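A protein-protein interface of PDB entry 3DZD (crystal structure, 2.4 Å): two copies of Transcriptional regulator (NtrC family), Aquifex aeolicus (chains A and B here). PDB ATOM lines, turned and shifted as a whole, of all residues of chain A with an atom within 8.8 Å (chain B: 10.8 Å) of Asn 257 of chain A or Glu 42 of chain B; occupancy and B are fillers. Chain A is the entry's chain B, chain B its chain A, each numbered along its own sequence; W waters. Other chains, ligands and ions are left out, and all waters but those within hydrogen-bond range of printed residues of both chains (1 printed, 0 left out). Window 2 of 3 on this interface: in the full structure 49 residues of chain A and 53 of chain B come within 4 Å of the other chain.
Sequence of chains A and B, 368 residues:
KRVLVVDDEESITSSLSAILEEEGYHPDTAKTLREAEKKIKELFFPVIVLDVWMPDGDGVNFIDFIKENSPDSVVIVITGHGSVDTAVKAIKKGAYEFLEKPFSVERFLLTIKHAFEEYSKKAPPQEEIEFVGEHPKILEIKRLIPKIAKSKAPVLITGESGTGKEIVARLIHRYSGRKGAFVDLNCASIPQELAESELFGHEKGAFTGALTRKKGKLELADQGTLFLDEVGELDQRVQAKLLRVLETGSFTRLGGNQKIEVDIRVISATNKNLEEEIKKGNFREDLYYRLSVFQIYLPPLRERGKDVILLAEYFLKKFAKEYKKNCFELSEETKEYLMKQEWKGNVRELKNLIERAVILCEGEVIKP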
ATOM      1  N   GLU A 203      10.143  -2.352  25.487  1.00  0.00           N
ATOM      2  CA  GLU A 203       9.811  -3.781  25.477  1.00  0.00           C
ATOM      3  C   GLU A 203      10.660  -4.672  24.563  1.00  0.00           C
ATOM      4  O   GLU A 203      11.453  -5.479  25.049  1.00  0.00           O
ATOM      5  CB  GLU A 203       8.315  -4.014  25.225  1.00  0.00           C
ATOM      6  CG  GLU A 203       7.513  -2.767  24.917  1.00  0.00           C
ATOM      7  CD  GLU A 203       6.202  -2.745  25.680  1.00  0.00           C
ATOM      8  OE1 GLU A 203       5.998  -3.635  26.530  1.00  0.00           O
ATOM      9  OE2 GLU A 203       5.377  -1.841  25.442  1.00  0.00           O
ATOM     10  N   PHE A 251       0.891   7.584  28.613  1.00  0.00           N
ATOM     11  CA  PHE A 251       2.018   7.417  27.703  1.00  0.00           C
ATOM     12  C   PHE A 251       2.083   6.001  27.138  1.00  0.00           C
ATOM     13  O   PHE A 251       1.293   5.134  27.503  1.00  0.00           O
ATOM     14  CB  PHE A 251       3.327   7.738  28.430  1.00  0.00           C
ATOM     15  CG  PHE A 251       3.663   6.769  29.533  1.00  0.00           C
ATOM     16  CD1 PHE A 251       4.692   5.850  29.379  1.00  0.00           C
ATOM     17  CD2 PHE A 251       2.945   6.770  30.719  1.00  0.00           C
ATOM     18  CE1 PHE A 251       5.009   4.959  30.389  1.00  0.00           C
ATOM     19  CE2 PHE A 251       3.250   5.873  31.729  1.00  0.00           C
ATOM     20  CZ  PHE A 251       4.288   4.967  31.566  1.00  0.00           C
ATOM     21  N   THR A 252       3.029   5.776  26.240  1.00  0.00           N
ATOM     22  CA  THR A 252       3.336   4.431  25.788  1.00  0.00           C
ATOM     23  C   THR A 252       4.808   4.204  26.062  1.00  0.00           C
ATOM     24  O   THR A 252       5.574   5.163  26.161  1.00  0.00           O
ATOM     25  CB  THR A 252       3.057   4.257  24.286  1.00  0.00           C
ATOM     26  OG1 THR A 252       3.591   5.373  23.567  1.00  0.00           O
ATOM     27  CG2 THR A 252       1.566   4.181  24.029  1.00  0.00           C
ATOM     28  N   ARG A 253       5.211   2.949  26.207  1.00  0.00           N
ATOM     29  CA  ARG A 253       6.628   2.663  26.356  1.00  0.00           C
ATOM     30  C   ARG A 253       7.291   2.812  24.999  1.00  0.00           C
ATOM     31  O   ARG A 253       6.613   2.996  23.985  1.00  0.00           O
ATOM     32  CB  ARG A 253       6.858   1.256  26.904  1.00  0.00           C
ATOM     33  CG  ARG A 253       6.431   1.076  28.345  1.00  0.00           C
ATOM     34  CD  ARG A 253       7.019  -0.190  28.922  1.00  0.00           C
ATOM     35  NE  ARG A 253       6.328  -0.623  30.132  1.00  0.00           N
ATOM     36  CZ  ARG A 253       5.171  -1.280  30.142  1.00  0.00           C
ATOM     37  NH1 ARG A 253       4.559  -1.573  28.998  1.00  0.00           N
ATOM     38  NH2 ARG A 253       4.619  -1.638  31.296  1.00  0.00           N
ATOM     39  N   LEU A 254       8.617   2.745  24.978  1.00  0.00           N
ATOM     40  CA  LEU A 254       9.346   2.737  23.718  1.00  0.00           C
ATOM     41  C   LEU A 254       9.168   1.373  23.064  1.00  0.00           C
ATOM     42  O   LEU A 254       9.409   0.339  23.686  1.00  0.00           O
ATOM     43  CB  LEU A 254      10.829   3.037  23.945  1.00  0.00           C
ATOM     44  CG  LEU A 254      11.158   4.387  24.587  1.00  0.00           C
ATOM     45  CD1 LEU A 254      12.664   4.635  24.605  1.00  0.00           C
ATOM     46  CD2 LEU A 254      10.432   5.510  23.862  1.00  0.00           C
ATOM     47  N   GLY A 255       8.734   1.370  21.809  1.00  0.00           N
ATOM     48  CA  GLY A 255       8.492   0.126  21.106  1.00  0.00           C
ATOM     49  C   GLY A 255       7.202  -0.489  21.595  1.00  0.00           C
ATOM     50  O   GLY A 255       7.015  -1.704  21.567  1.00  0.00           O
ATOM     51  N   GLY A 256       6.310   0.373  22.064  1.00  0.00           N
ATOM     52  CA  GLY A 256       5.027  -0.059  22.570  1.00  0.00           C
ATOM     53  C   GLY A 256       3.935   0.869  22.093  1.00  0.00           C
ATOM     54  O   GLY A 256       4.177   2.046  21.816  1.00  0.00           O
ATOM     55  N   ASN A 257       2.726   0.335  21.998  1.00  0.00           N
ATOM     56  CA  ASN A 257       1.598   1.118  21.530  1.00  0.00           C
ATOM     57  C   ASN A 257       0.474   1.123  22.560  1.00  0.00           C
ATOM     58  O   ASN A 257      -0.517   1.843  22.423  1.00  0.00           O
ATOM     59  CB  ASN A 257       1.110   0.579  20.187  1.00  0.00           C
ATOM     60  CG  ASN A 257       0.826   1.682  19.195  1.00  0.00           C
ATOM     61  OD1 ASN A 257       0.377   2.766  19.569  1.00  0.00           O
ATOM     62  ND2 ASN A 257       1.095   1.417  17.921  1.00  0.00           N
ATOM     63  N   GLN A 258       0.644   0.315  23.601  1.00  0.00           N
ATOM     64  CA  GLN A 258      -0.334   0.241  24.675  1.00  0.00           C
ATOM     65  C   GLN A 258      -0.339   1.513  25.506  1.00  0.00           C
ATOM     66  O   GLN A 258       0.691   1.929  26.037  1.00  0.00           O
ATOM     67  CB  GLN A 258      -0.048  -0.950  25.574  1.00  0.00           C
ATOM     68  CG  GLN A 258      -1.112  -1.181  26.611  1.00  0.00           C
ATOM     69  CD  GLN A 258      -0.767  -2.320  27.530  1.00  0.00           C
ATOM     70  OE1 GLN A 258       0.320  -2.355  28.111  1.00  0.00           O
ATOM     71  NE2 GLN A 258      -1.692  -3.266  27.673  1.00  0.00           N
ATOM     72  N   LYS A 259      -1.510   2.125  25.616  1.00  0.00           N
ATOM     73  CA  LYS A 259      -1.651   3.385  26.333  1.00  0.00           C
ATOM     74  C   LYS A 259      -1.698   3.120  27.837  1.00  0.00           C
ATOM     75  O   LYS A 259      -2.552   2.373  28.321  1.00  0.00           O
ATOM     76  CB  LYS A 259      -2.913   4.106  25.851  1.00  0.00           C
ATOM     77  CG  LYS A 259      -3.110   5.514  26.386  1.00  0.00           C
ATOM     78  CD  LYS A 259      -4.288   6.176  25.693  1.00  0.00           C
ATOM     79  CE  LYS A 259      -4.703   7.469  26.375  1.00  0.00           C
ATOM     80  NZ  LYS A 259      -5.524   7.224  27.591  1.00  0.00           N
ATOM     81  N   ILE A 260      -0.764   3.721  28.567  1.00  0.00           N
ATOM     82  CA  ILE A 260      -0.666   3.535  30.014  1.00  0.00           C
ATOM     83  C   ILE A 260      -0.941   4.830  30.783  1.00  0.00           C
ATOM     84  O   ILE A 260      -0.388   5.881  30.466  1.00  0.00           O
ATOM     85  CB  ILE A 260       0.708   2.992  30.411  1.00  0.00           C
ATOM     86  CG1 ILE A 260       1.044   1.741  29.594  1.00  0.00           C
ATOM     87  CG2 ILE A 260       0.748   2.687  31.912  1.00  0.00           C
ATOM     88  CD1 ILE A 260       2.411   1.159  29.896  1.00  0.00           C
ATOM     89  N   GLU A 261      -1.792   4.764  31.801  1.00  0.00           N
ATOM     90  CA  GLU A 261      -2.178   5.980  32.508  1.00  0.00           C
ATOM     91  C   GLU A 261      -1.537   6.105  33.879  1.00  0.00           C
ATOM     92  O   GLU A 261      -1.549   5.162  34.666  1.00  0.00           O
ATOM     93  CB  GLU A 261      -3.697   6.092  32.606  1.00  0.00           C
ATOM     94  CG  GLU A 261      -4.350   6.365  31.267  1.00  0.00           C
ATOM     95  CD  GLU A 261      -5.858   6.262  31.317  1.00  0.00           C
ATOM     96  OE1 GLU A 261      -6.408   6.100  32.427  1.00  0.00           O
ATOM     97  OE2 GLU A 261      -6.489   6.344  30.244  1.00  0.00           O
ATOM     98  N   ARG B   2      -8.983   1.968  35.737  1.00  0.00           N
ATOM     99  CA  ARG B   2      -9.709   1.257  34.690  1.00  0.00           C
ATOM    100  C   ARG B   2      -9.970  -0.208  35.023  1.00  0.00           C
ATOM    101  O   ARG B   2      -9.193  -0.843  35.730  1.00  0.00           O
ATOM    102  CB  ARG B   2      -8.973   1.360  33.361  1.00  0.00           C
ATOM    103  CG  ARG B   2      -8.984   2.746  32.765  1.00  0.00           C
ATOM    104  CD  ARG B   2      -8.698   2.682  31.283  1.00  0.00           C
ATOM    105  NE  ARG B   2      -8.581   4.002  30.670  1.00  0.00           N
ATOM    106  CZ  ARG B   2      -9.590   4.856  30.530  1.00  0.00           C
ATOM    107  NH1 ARG B   2     -10.802   4.547  30.977  1.00  0.00           N
ATOM    108  NH2 ARG B   2      -9.383   6.030  29.949  1.00  0.00           N
ATOM    109  N   LEU B   4     -11.452  -3.706  32.828  1.00  0.00           N
ATOM    110  CA  LEU B   4     -12.030  -4.307  31.630  1.00  0.00           C
ATOM    111  C   LEU B   4     -12.861  -5.513  32.017  1.00  0.00           C
ATOM    112  O   LEU B   4     -12.367  -6.423  32.683  1.00  0.00           O
ATOM    113  CB  LEU B   4     -10.946  -4.724  30.625  1.00  0.00           C
ATOM    114  CG  LEU B   4     -11.426  -5.532  29.408  1.00  0.00           C
ATOM    115  CD1 LEU B   4     -12.290  -4.687  28.472  1.00  0.00           C
ATOM    116  CD2 LEU B   4     -10.253  -6.136  28.649  1.00  0.00           C
ATOM    117  N   ASP B  28     -14.780  -0.601  31.183  1.00  0.00           N
ATOM    118  CA  ASP B  28     -14.955  -0.843  29.758  1.00  0.00           C
ATOM    119  C   ASP B  28     -15.364  -2.303  29.632  1.00  0.00           C
ATOM    120  O   ASP B  28     -15.168  -3.074  30.563  1.00  0.00           O
ATOM    121  CB  ASP B  28     -13.655  -0.588  29.002  1.00  0.00           C
ATOM    122  CG  ASP B  28     -13.878  -0.331  27.520  1.00  0.00           C
ATOM    123  OD1 ASP B  28     -15.014  -0.536  27.028  1.00  0.00           O
ATOM    124  OD2 ASP B  28     -12.907   0.079  26.846  1.00  0.00           O
ATOM    125  N   THR B  29     -15.938  -2.688  28.497  1.00  0.00           N
ATOM    126  CA  THR B  29     -16.425  -4.052  28.333  1.00  0.00           C
ATOM    127  C   THR B  29     -16.073  -4.631  26.973  1.00  0.00           C
ATOM    128  O   THR B  29     -16.081  -3.925  25.969  1.00  0.00           O
ATOM    129  CB  THR B  29     -17.949  -4.134  28.526  1.00  0.00           C
ATOM    130  OG1 THR B  29     -18.602  -3.356  27.520  1.00  0.00           O
ATOM    131  CG2 THR B  29     -18.345  -3.600  29.889  1.00  0.00           C
ATOM    132  N   ALA B  30     -15.756  -5.921  26.955  1.00  0.00           N
ATOM    133  CA  ALA B  30     -15.541  -6.658  25.717  1.00  0.00           C
ATOM    134  C   ALA B  30     -16.465  -7.868  25.700  1.00  0.00           C
ATOM    135  O   ALA B  30     -16.554  -8.602  26.683  1.00  0.00           O
ATOM    136  CB  ALA B  30     -14.099  -7.093  25.598  1.00  0.00           C
ATOM    137  N   ARG B  34     -12.145 -11.721  20.906  1.00  0.00           N
ATOM    138  CA  ARG B  34     -11.603 -10.901  19.833  1.00  0.00           C
ATOM    139  C   ARG B  34     -11.577  -9.436  20.243  1.00  0.00           C
ATOM    140  O   ARG B  34     -10.528  -8.798  20.223  1.00  0.00           O
ATOM    141  CB  ARG B  34     -12.425 -11.069  18.558  1.00  0.00           C
ATOM    142  CG  ARG B  34     -11.892 -10.286  17.375  1.00  0.00           C
ATOM    143  CD  ARG B  34     -12.656 -10.643  16.116  1.00  0.00           C
ATOM    144  NE  ARG B  34     -12.246  -9.849  14.963  1.00  0.00           N
ATOM    145  CZ  ARG B  34     -11.389 -10.261  14.035  1.00  0.00           C
ATOM    146  NH1 ARG B  34     -10.837 -11.464  14.124  1.00  0.00           N
ATOM    147  NH2 ARG B  34     -11.083  -9.469  13.015  1.00  0.00           N
ATOM    148  N   GLU B  35     -12.741  -8.912  20.610  1.00  0.00           N
ATOM    149  CA  GLU B  35     -12.867  -7.524  21.041  1.00  0.00           C
ATOM    150  C   GLU B  35     -11.953  -7.233  22.231  1.00  0.00           C
ATOM    151  O   GLU B  35     -11.399  -6.142  22.357  1.00  0.00           O
ATOM    152  CB  GLU B  35     -14.321  -7.225  21.405  1.00  0.00           C
ATOM    153  CG  GLU B  35     -14.648  -5.755  21.575  1.00  0.00           C
ATOM    154  CD  GLU B  35     -16.049  -5.532  22.128  1.00  0.00           C
ATOM    155  OE1 GLU B  35     -16.889  -6.454  22.018  1.00  0.00           O
ATOM    156  OE2 GLU B  35     -16.312  -4.437  22.674  1.00  0.00           O
ATOM    157  N   ALA B  36     -11.788  -8.217  23.105  1.00  0.00           N
ATOM    158  CA  ALA B  36     -10.958  -8.022  24.278  1.00  0.00           C
ATOM    159  C   ALA B  36      -9.512  -7.790  23.864  1.00  0.00           C
ATOM    160  O   ALA B  36      -8.901  -6.799  24.265  1.00  0.00           O
ATOM    161  CB  ALA B  36     -11.068  -9.211  25.217  1.00  0.00           C
ATOM    162  N   GLU B  37      -8.971  -8.704  23.061  1.00  0.00           N
ATOM    163  CA  GLU B  37      -7.588  -8.608  22.594  1.00  0.00           C
ATOM    164  C   GLU B  37      -7.304  -7.228  22.029  1.00  0.00           C
ATOM    165  O   GLU B  37      -6.249  -6.642  22.272  1.00  0.00           O
ATOM    166  CB  GLU B  37      -7.310  -9.668  21.532  1.00  0.00           C
ATOM    167  CG  GLU B  37      -7.408 -11.085  22.054  1.00  0.00           C
ATOM    168  CD  GLU B  37      -7.238 -12.123  20.965  1.00  0.00           C
ATOM    169  OE1 GLU B  37      -7.493 -11.799  19.785  1.00  0.00           O
ATOM    170  OE2 GLU B  37      -6.857 -13.268  21.293  1.00  0.00           O
ATOM    171  N   LYS B  38      -8.261  -6.716  21.270  1.00  0.00           N
ATOM    172  CA  LYS B  38      -8.185  -5.366  20.745  1.00  0.00           C
ATOM    173  C   LYS B  38      -7.879  -4.393  21.877  1.00  0.00           C
ATOM    174  O   LYS B  38      -6.836  -3.731  21.884  1.00  0.00           O
ATOM    175  CB  LYS B  38      -9.515  -5.003  20.084  1.00  0.00           C
ATOM    176  CG  LYS B  38      -9.725  -3.524  19.821  1.00  0.00           C
ATOM    177  CD  LYS B  38      -9.011  -3.081  18.565  1.00  0.00           C
ATOM    178  CE  LYS B  38      -9.609  -1.792  18.045  1.00  0.00           C
ATOM    179  NZ  LYS B  38      -9.758  -0.799  19.144  1.00  0.00           N
ATOM    180  N   LYS B  39      -8.784  -4.323  22.847  1.00  0.00           N
ATOM    181  CA  LYS B  39      -8.679  -3.324  23.905  1.00  0.00           C
ATOM    182  C   LYS B  39      -7.452  -3.489  24.806  1.00  0.00           C
ATOM    183  O   LYS B  39      -6.893  -2.502  25.286  1.00  0.00           O
ATOM    184  CB  LYS B  39      -9.977  -3.259  24.713  1.00  0.00           C
ATOM    185  CG  LYS B  39     -11.028  -2.404  24.030  1.00  0.00           C
ATOM    186  CD  LYS B  39     -12.435  -2.703  24.493  1.00  0.00           C
ATOM    187  CE  LYS B  39     -13.395  -1.717  23.857  1.00  0.00           C
ATOM    188  NZ  LYS B  39     -14.793  -2.166  23.981  1.00  0.00           N
ATOM    189  N   ILE B  40      -7.024  -4.726  25.018  1.00  0.00           N
ATOM    190  CA  ILE B  40      -5.870  -4.990  25.873  1.00  0.00           C
ATOM    191  C   ILE B  40      -4.582  -4.431  25.259  1.00  0.00           C
ATOM    192  O   ILE B  40      -3.804  -3.751  25.934  1.00  0.00           O
ATOM    193  CB  ILE B  40      -5.735  -6.503  26.163  1.00  0.00           C
ATOM    194  CG1 ILE B  40      -6.901  -6.975  27.034  1.00  0.00           C
ATOM    195  CG2 ILE B  40      -4.409  -6.818  26.819  1.00  0.00           C
ATOM    196  CD1 ILE B  40      -6.937  -8.464  27.254  1.00  0.00           C
ATOM    197  N   LYS B  41      -4.374  -4.706  23.974  1.00  0.00           N
ATOM    198  CA  LYS B  41      -3.181  -4.253  23.262  1.00  0.00           C
ATOM    199  C   LYS B  41      -3.201  -2.739  23.093  1.00  0.00           C
ATOM    200  O   LYS B  41      -2.161  -2.100  22.925  1.00  0.00           O
ATOM    201  CB  LYS B  41      -3.096  -4.928  21.888  1.00  0.00           C
ATOM    202  CG  LYS B  41      -2.895  -6.436  21.944  1.00  0.00           C
ATOM    203  CD  LYS B  41      -3.417  -7.126  20.694  1.00  0.00           C
ATOM    204  CE  LYS B  41      -2.618  -6.735  19.462  1.00  0.00           C
ATOM    205  NZ  LYS B  41      -3.158  -7.357  18.218  1.00  0.00           N
ATOM    206  N   GLU B  42      -4.402  -2.179  23.148  1.00  0.00           N
ATOM    207  CA  GLU B  42      -4.631  -0.768  22.885  1.00  0.00           C
ATOM    208  C   GLU B  42      -4.418   0.073  24.143  1.00  0.00           C
ATOM    209  O   GLU B  42      -3.858   1.172  24.089  1.00  0.00           O
ATOM    210  CB  GLU B  42      -6.062  -0.598  22.373  1.00  0.00           C
ATOM    211  CG  GLU B  42      -6.425   0.781  21.856  1.00  0.00           C
ATOM    212  CD  GLU B  42      -7.878   0.856  21.407  1.00  0.00           C
ATOM    213  OE1 GLU B  42      -8.762   0.370  22.149  1.00  0.00           O
ATOM    214  OE2 GLU B  42      -8.135   1.396  20.311  1.00  0.00           O
ATOM    215  N   LEU B  43      -4.859  -0.455  25.281  1.00  0.00           N
ATOM    216  CA  LEU B  43      -4.869   0.307  26.520  1.00  0.00           C
ATOM    217  C   LEU B  43      -4.638  -0.602  27.728  1.00  0.00           C
ATOM    218  O   LEU B  43      -5.026  -1.771  27.729  1.00  0.00           O
ATOM    219  CB  LEU B  43      -6.188   1.073  26.637  1.00  0.00           C
ATOM    220  CG  LEU B  43      -6.706   1.523  28.005  1.00  0.00           C
ATOM    221  CD1 LEU B  43      -5.788   2.565  28.640  1.00  0.00           C
ATOM    222  CD2 LEU B  43      -8.119   2.071  27.862  1.00  0.00           C
ATOM    223  N   PHE B  44      -3.978  -0.071  28.750  1.00  0.00           N
ATOM    224  CA  PHE B  44      -3.664  -0.875  29.923  1.00  0.00           C
ATOM    225  C   PHE B  44      -4.757  -0.840  30.992  1.00  0.00           C
ATOM    226  O   PHE B  44      -5.096   0.223  31.512  1.00  0.00           O
ATOM    227  CB  PHE B  44      -2.332  -0.456  30.543  1.00  0.00           C
ATOM    228  CG  PHE B  44      -2.008  -1.202  31.803  1.00  0.00           C
ATOM    229  CD1 PHE B  44      -1.599  -2.523  31.750  1.00  0.00           C
ATOM    230  CD2 PHE B  44      -2.149  -0.598  33.039  1.00  0.00           C
ATOM    231  CE1 PHE B  44      -1.318  -3.218  32.897  1.00  0.00           C
ATOM    232  CE2 PHE B  44      -1.868  -1.293  34.194  1.00  0.00           C
ATOM    233  CZ  PHE B  44      -1.450  -2.606  34.123  1.00  0.00           C
ATOM    234  N   PHE B  45      -5.304  -2.013  31.306  1.00  0.00           N
ATOM    235  CA  PHE B  45      -6.243  -2.155  32.416  1.00  0.00           C
ATOM    236  C   PHE B  45      -5.535  -2.831  33.575  1.00  0.00           C
ATOM    237  O   PHE B  45      -5.097  -3.966  33.443  1.00  0.00           O
ATOM    238  CB  PHE B  45      -7.444  -3.008  32.010  1.00  0.00           C
ATOM    239  CG  PHE B  45      -8.238  -2.441  30.872  1.00  0.00           C
ATOM    240  CD1 PHE B  45      -9.214  -1.483  31.099  1.00  0.00           C
ATOM    241  CD2 PHE B  45      -8.024  -2.881  29.575  1.00  0.00           C
ATOM    242  CE1 PHE B  45      -9.953  -0.965  30.053  1.00  0.00           C
ATOM    243  CE2 PHE B  45      -8.757  -2.368  28.522  1.00  0.00           C
ATOM    244  CZ  PHE B  45      -9.725  -1.410  28.762  1.00  0.00           C
ATOM    245  N   ILE B  48      -8.596  -6.890  35.143  1.00  0.00           N
ATOM    246  CA  ILE B  48      -9.426  -7.475  34.112  1.00  0.00           C
ATOM    247  C   ILE B  48     -10.296  -8.540  34.732  1.00  0.00           C
ATOM    248  O   ILE B  48      -9.806  -9.383  35.487  1.00  0.00           O
ATOM    249  CB  ILE B  48      -8.587  -8.108  33.012  1.00  0.00           C
ATOM    250  CG1 ILE B  48      -7.771  -7.031  32.293  1.00  0.00           C
ATOM    251  CG2 ILE B  48      -9.477  -8.853  32.038  1.00  0.00           C
ATOM    252  CD1 ILE B  48      -6.704  -7.582  31.379  1.00  0.00           C
ATOM    253  N   PHE B  62      -7.186 -17.857  27.623  1.00  0.00           N
ATOM    254  CA  PHE B  62      -7.037 -16.443  27.292  1.00  0.00           C
ATOM    255  C   PHE B  62      -6.205 -15.705  28.336  1.00  0.00           C
ATOM    256  O   PHE B  62      -5.620 -14.663  28.055  1.00  0.00           O
ATOM    257  CB  PHE B  62      -8.398 -15.769  27.152  1.00  0.00           C
ATOM    258  CG  PHE B  62      -8.318 -14.367  26.638  1.00  0.00           C
ATOM    259  CD1 PHE B  62      -8.161 -14.122  25.284  1.00  0.00           C
ATOM    260  CD2 PHE B  62      -8.385 -13.291  27.506  1.00  0.00           C
ATOM    261  CE1 PHE B  62      -8.080 -12.830  24.802  1.00  0.00           C
ATOM    262  CE2 PHE B  62      -8.302 -11.994  27.028  1.00  0.00           C
ATOM    263  CZ  PHE B  62      -8.152 -11.766  25.671  1.00  0.00           C
ATOM    264  N   PHE B  65      -2.977 -14.999  26.970  1.00  0.00           N
ATOM    265  CA  PHE B  65      -2.931 -13.798  26.151  1.00  0.00           C
ATOM    266  C   PHE B  65      -2.636 -12.578  27.012  1.00  0.00           C
ATOM    267  O   PHE B  65      -1.816 -11.736  26.652  1.00  0.00           O
ATOM    268  CB  PHE B  65      -4.249 -13.583  25.420  1.00  0.00           C
ATOM    269  CG  PHE B  65      -4.274 -12.329  24.601  1.00  0.00           C
ATOM    270  CD1 PHE B  65      -4.050 -12.375  23.236  1.00  0.00           C
ATOM    271  CD2 PHE B  65      -4.495 -11.099  25.198  1.00  0.00           C
ATOM    272  CE1 PHE B  65      -4.059 -11.223  22.480  1.00  0.00           C
ATOM    273  CE2 PHE B  65      -4.512  -9.942  24.445  1.00  0.00           C
ATOM    274  CZ  PHE B  65      -4.294 -10.005  23.084  1.00  0.00           C
ATOM    275  N   ASN B  69       0.548  -9.982  26.876  1.00  0.00           N
ATOM    276  CA  ASN B  69       0.441  -8.623  26.365  1.00  0.00           C
ATOM    277  C   ASN B  69       0.035  -7.571  27.402  1.00  0.00           C
ATOM    278  O   ASN B  69      -0.142  -6.399  27.066  1.00  0.00           O
ATOM    279  CB  ASN B  69      -0.527  -8.600  25.182  1.00  0.00           C
ATOM    280  CG  ASN B  69      -0.331  -9.786  24.250  1.00  0.00           C
ATOM    281  OD1 ASN B  69       0.734 -10.403  24.226  1.00  0.00           O
ATOM    282  ND2 ASN B  69      -1.361 -10.112  23.482  1.00  0.00           N
ATOM    283  N   SER B  70      -0.110  -7.987  28.658  1.00  0.00           N
ATOM    284  CA  SER B  70      -0.445  -7.066  29.743  1.00  0.00           C
ATOM    285  C   SER B  70      -0.091  -7.695  31.091  1.00  0.00           C
ATOM    286  O   SER B  70      -0.961  -7.896  31.940  1.00  0.00           O
ATOM    287  CB  SER B  70      -1.930  -6.701  29.693  1.00  0.00           C
ATOM    288  OG  SER B  70      -2.159  -5.425  30.263  1.00  0.00           O
ATOM    289  N   SER B  73      -1.459  -6.677  34.497  1.00  0.00           N
ATOM    290  CA  SER B  73      -2.887  -6.792  34.773  1.00  0.00           C
ATOM    291  C   SER B  73      -3.172  -7.886  35.798  1.00  0.00           C
ATOM    292  O   SER B  73      -2.622  -8.987  35.720  1.00  0.00           O
ATOM    293  CB  SER B  73      -3.675  -7.069  33.500  1.00  0.00           C
ATOM    294  OG  SER B  73      -3.790  -5.897  32.719  1.00  0.00           O
HETATM  295  O   HOH W   1      -4.352  -3.915  29.566  1.00  0.00           O
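The backbone carbonyl oxygen (O) of Glu 42 of chain B is in hydrogen-bond range of the backbone NH (N) of Lys 259 of chain A (3.0 Å). N of Phe 44 of chain B lies within hydrogen-bond range of O of Lys 259 of chain A (2.9 Å). OG of Ser 70 of chain B lies within hydrogen-bond range of NE2 of Gln 258 of chain A (3.4 Å). O of Ile 40 of chain B sits at hydrogen-bond distance from NE2 of Gln 258 of chain A (2.8 Å). The guanidinium group (NH2) of Arg 2 of chain B is in salt-bridge range of the side-chain carboxylate (OE2) of Glu 261 of chain A (2.9 Å).
The side-chain hydroxyl of Ser 73 of chain B sits at hydrogen-bond distance from the side-chain hydroxyl of Ser 70 of chain B, at 3.0 Å. NZ of Lys 38 of chain B is in salt-bridge range of OE2 of Glu 42 of chain B (3.0 Å). NZ of Lys 259 of chain A lies within salt-bridge range of OE2 of Glu 261 of chain A, 3.0 Å away.
Among the printed residues, pairs that only touch across the chains: Asn 257 of chain A with Glu 42 of chain B (3.8 Å), Gln 258 of chain A with Lys 41 of chain B (3.4 Å), Gln 258 of chain A with Glu 42 of chain B (3.7 Å), Gln 258 of chain A with Leu 43 of chain B (3.7 Å), Gln 258 of chain A with Phe 44 of chain B (3.7 Å), Gln 258 of chain A with Asn 69 of chain B (3.5 Å) and Lys 259 of chain A with Leu 43 of chain B (3.3 Å).
No residue of chain B comes within 4 Å of Gly 255 of chain A. No residue of chain B comes within 4 Å of Gly 256 of chain A. Of chain B, only Glu 42 (3.8 Å) comes within 4 Å of Asn 257 of chain A. Printed residues of chain B within 4 Å of Glu 261 of chain A: Arg 2 (2.9 Å). Glu 42 of chain B touches just these residues of chain A: Asn 257 (3.8 Å), Gln 258 (3.7 Å) and Lys 259 (3.0 Å). Ile 48 of chain B touches none of the printed residues of chain A. Phe 65 of chain B touches none of the printed residues of chain A. Of the printed residues of chain A, Asn 69 of chain B touches Gln 258. Of the printed residues of chain A, Ser 70 of chain B touches Gln 258. The nearest residue of chain B that does not touch Asn 257 of chain A is Lys 41 of chain B (4.2 Å). The nearest residue of chain A that does not touch Glu 42 of chain B is Ile 260 of chain A (6.0 Å). The nearest printed residue of chain A that does not touch Ser 70 of chain B is Arg 253 of chain A (7.5 Å).
Of the 23 printed residues of chain B, 8 touch a printed residue of chain A. Hydrophobic or aromatic side chains of chain B within 4 Å of the printed part of chain A: Leu 43 and Phe 44.
No position is printed for both chains. Of the 12 pairs that touch across the chains among the printed residues, none has its exchanged pair printed and touching as well.
Water W1 lies within hydrogen-bond range of N of Phe 45 of chain B (2.7 Å), OG of Ser 70 of chain B (2.8 Å), O of Leu 43 of chain B (2.9 Å) and NE2 of Gln 258 of chain A (3.3 Å).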
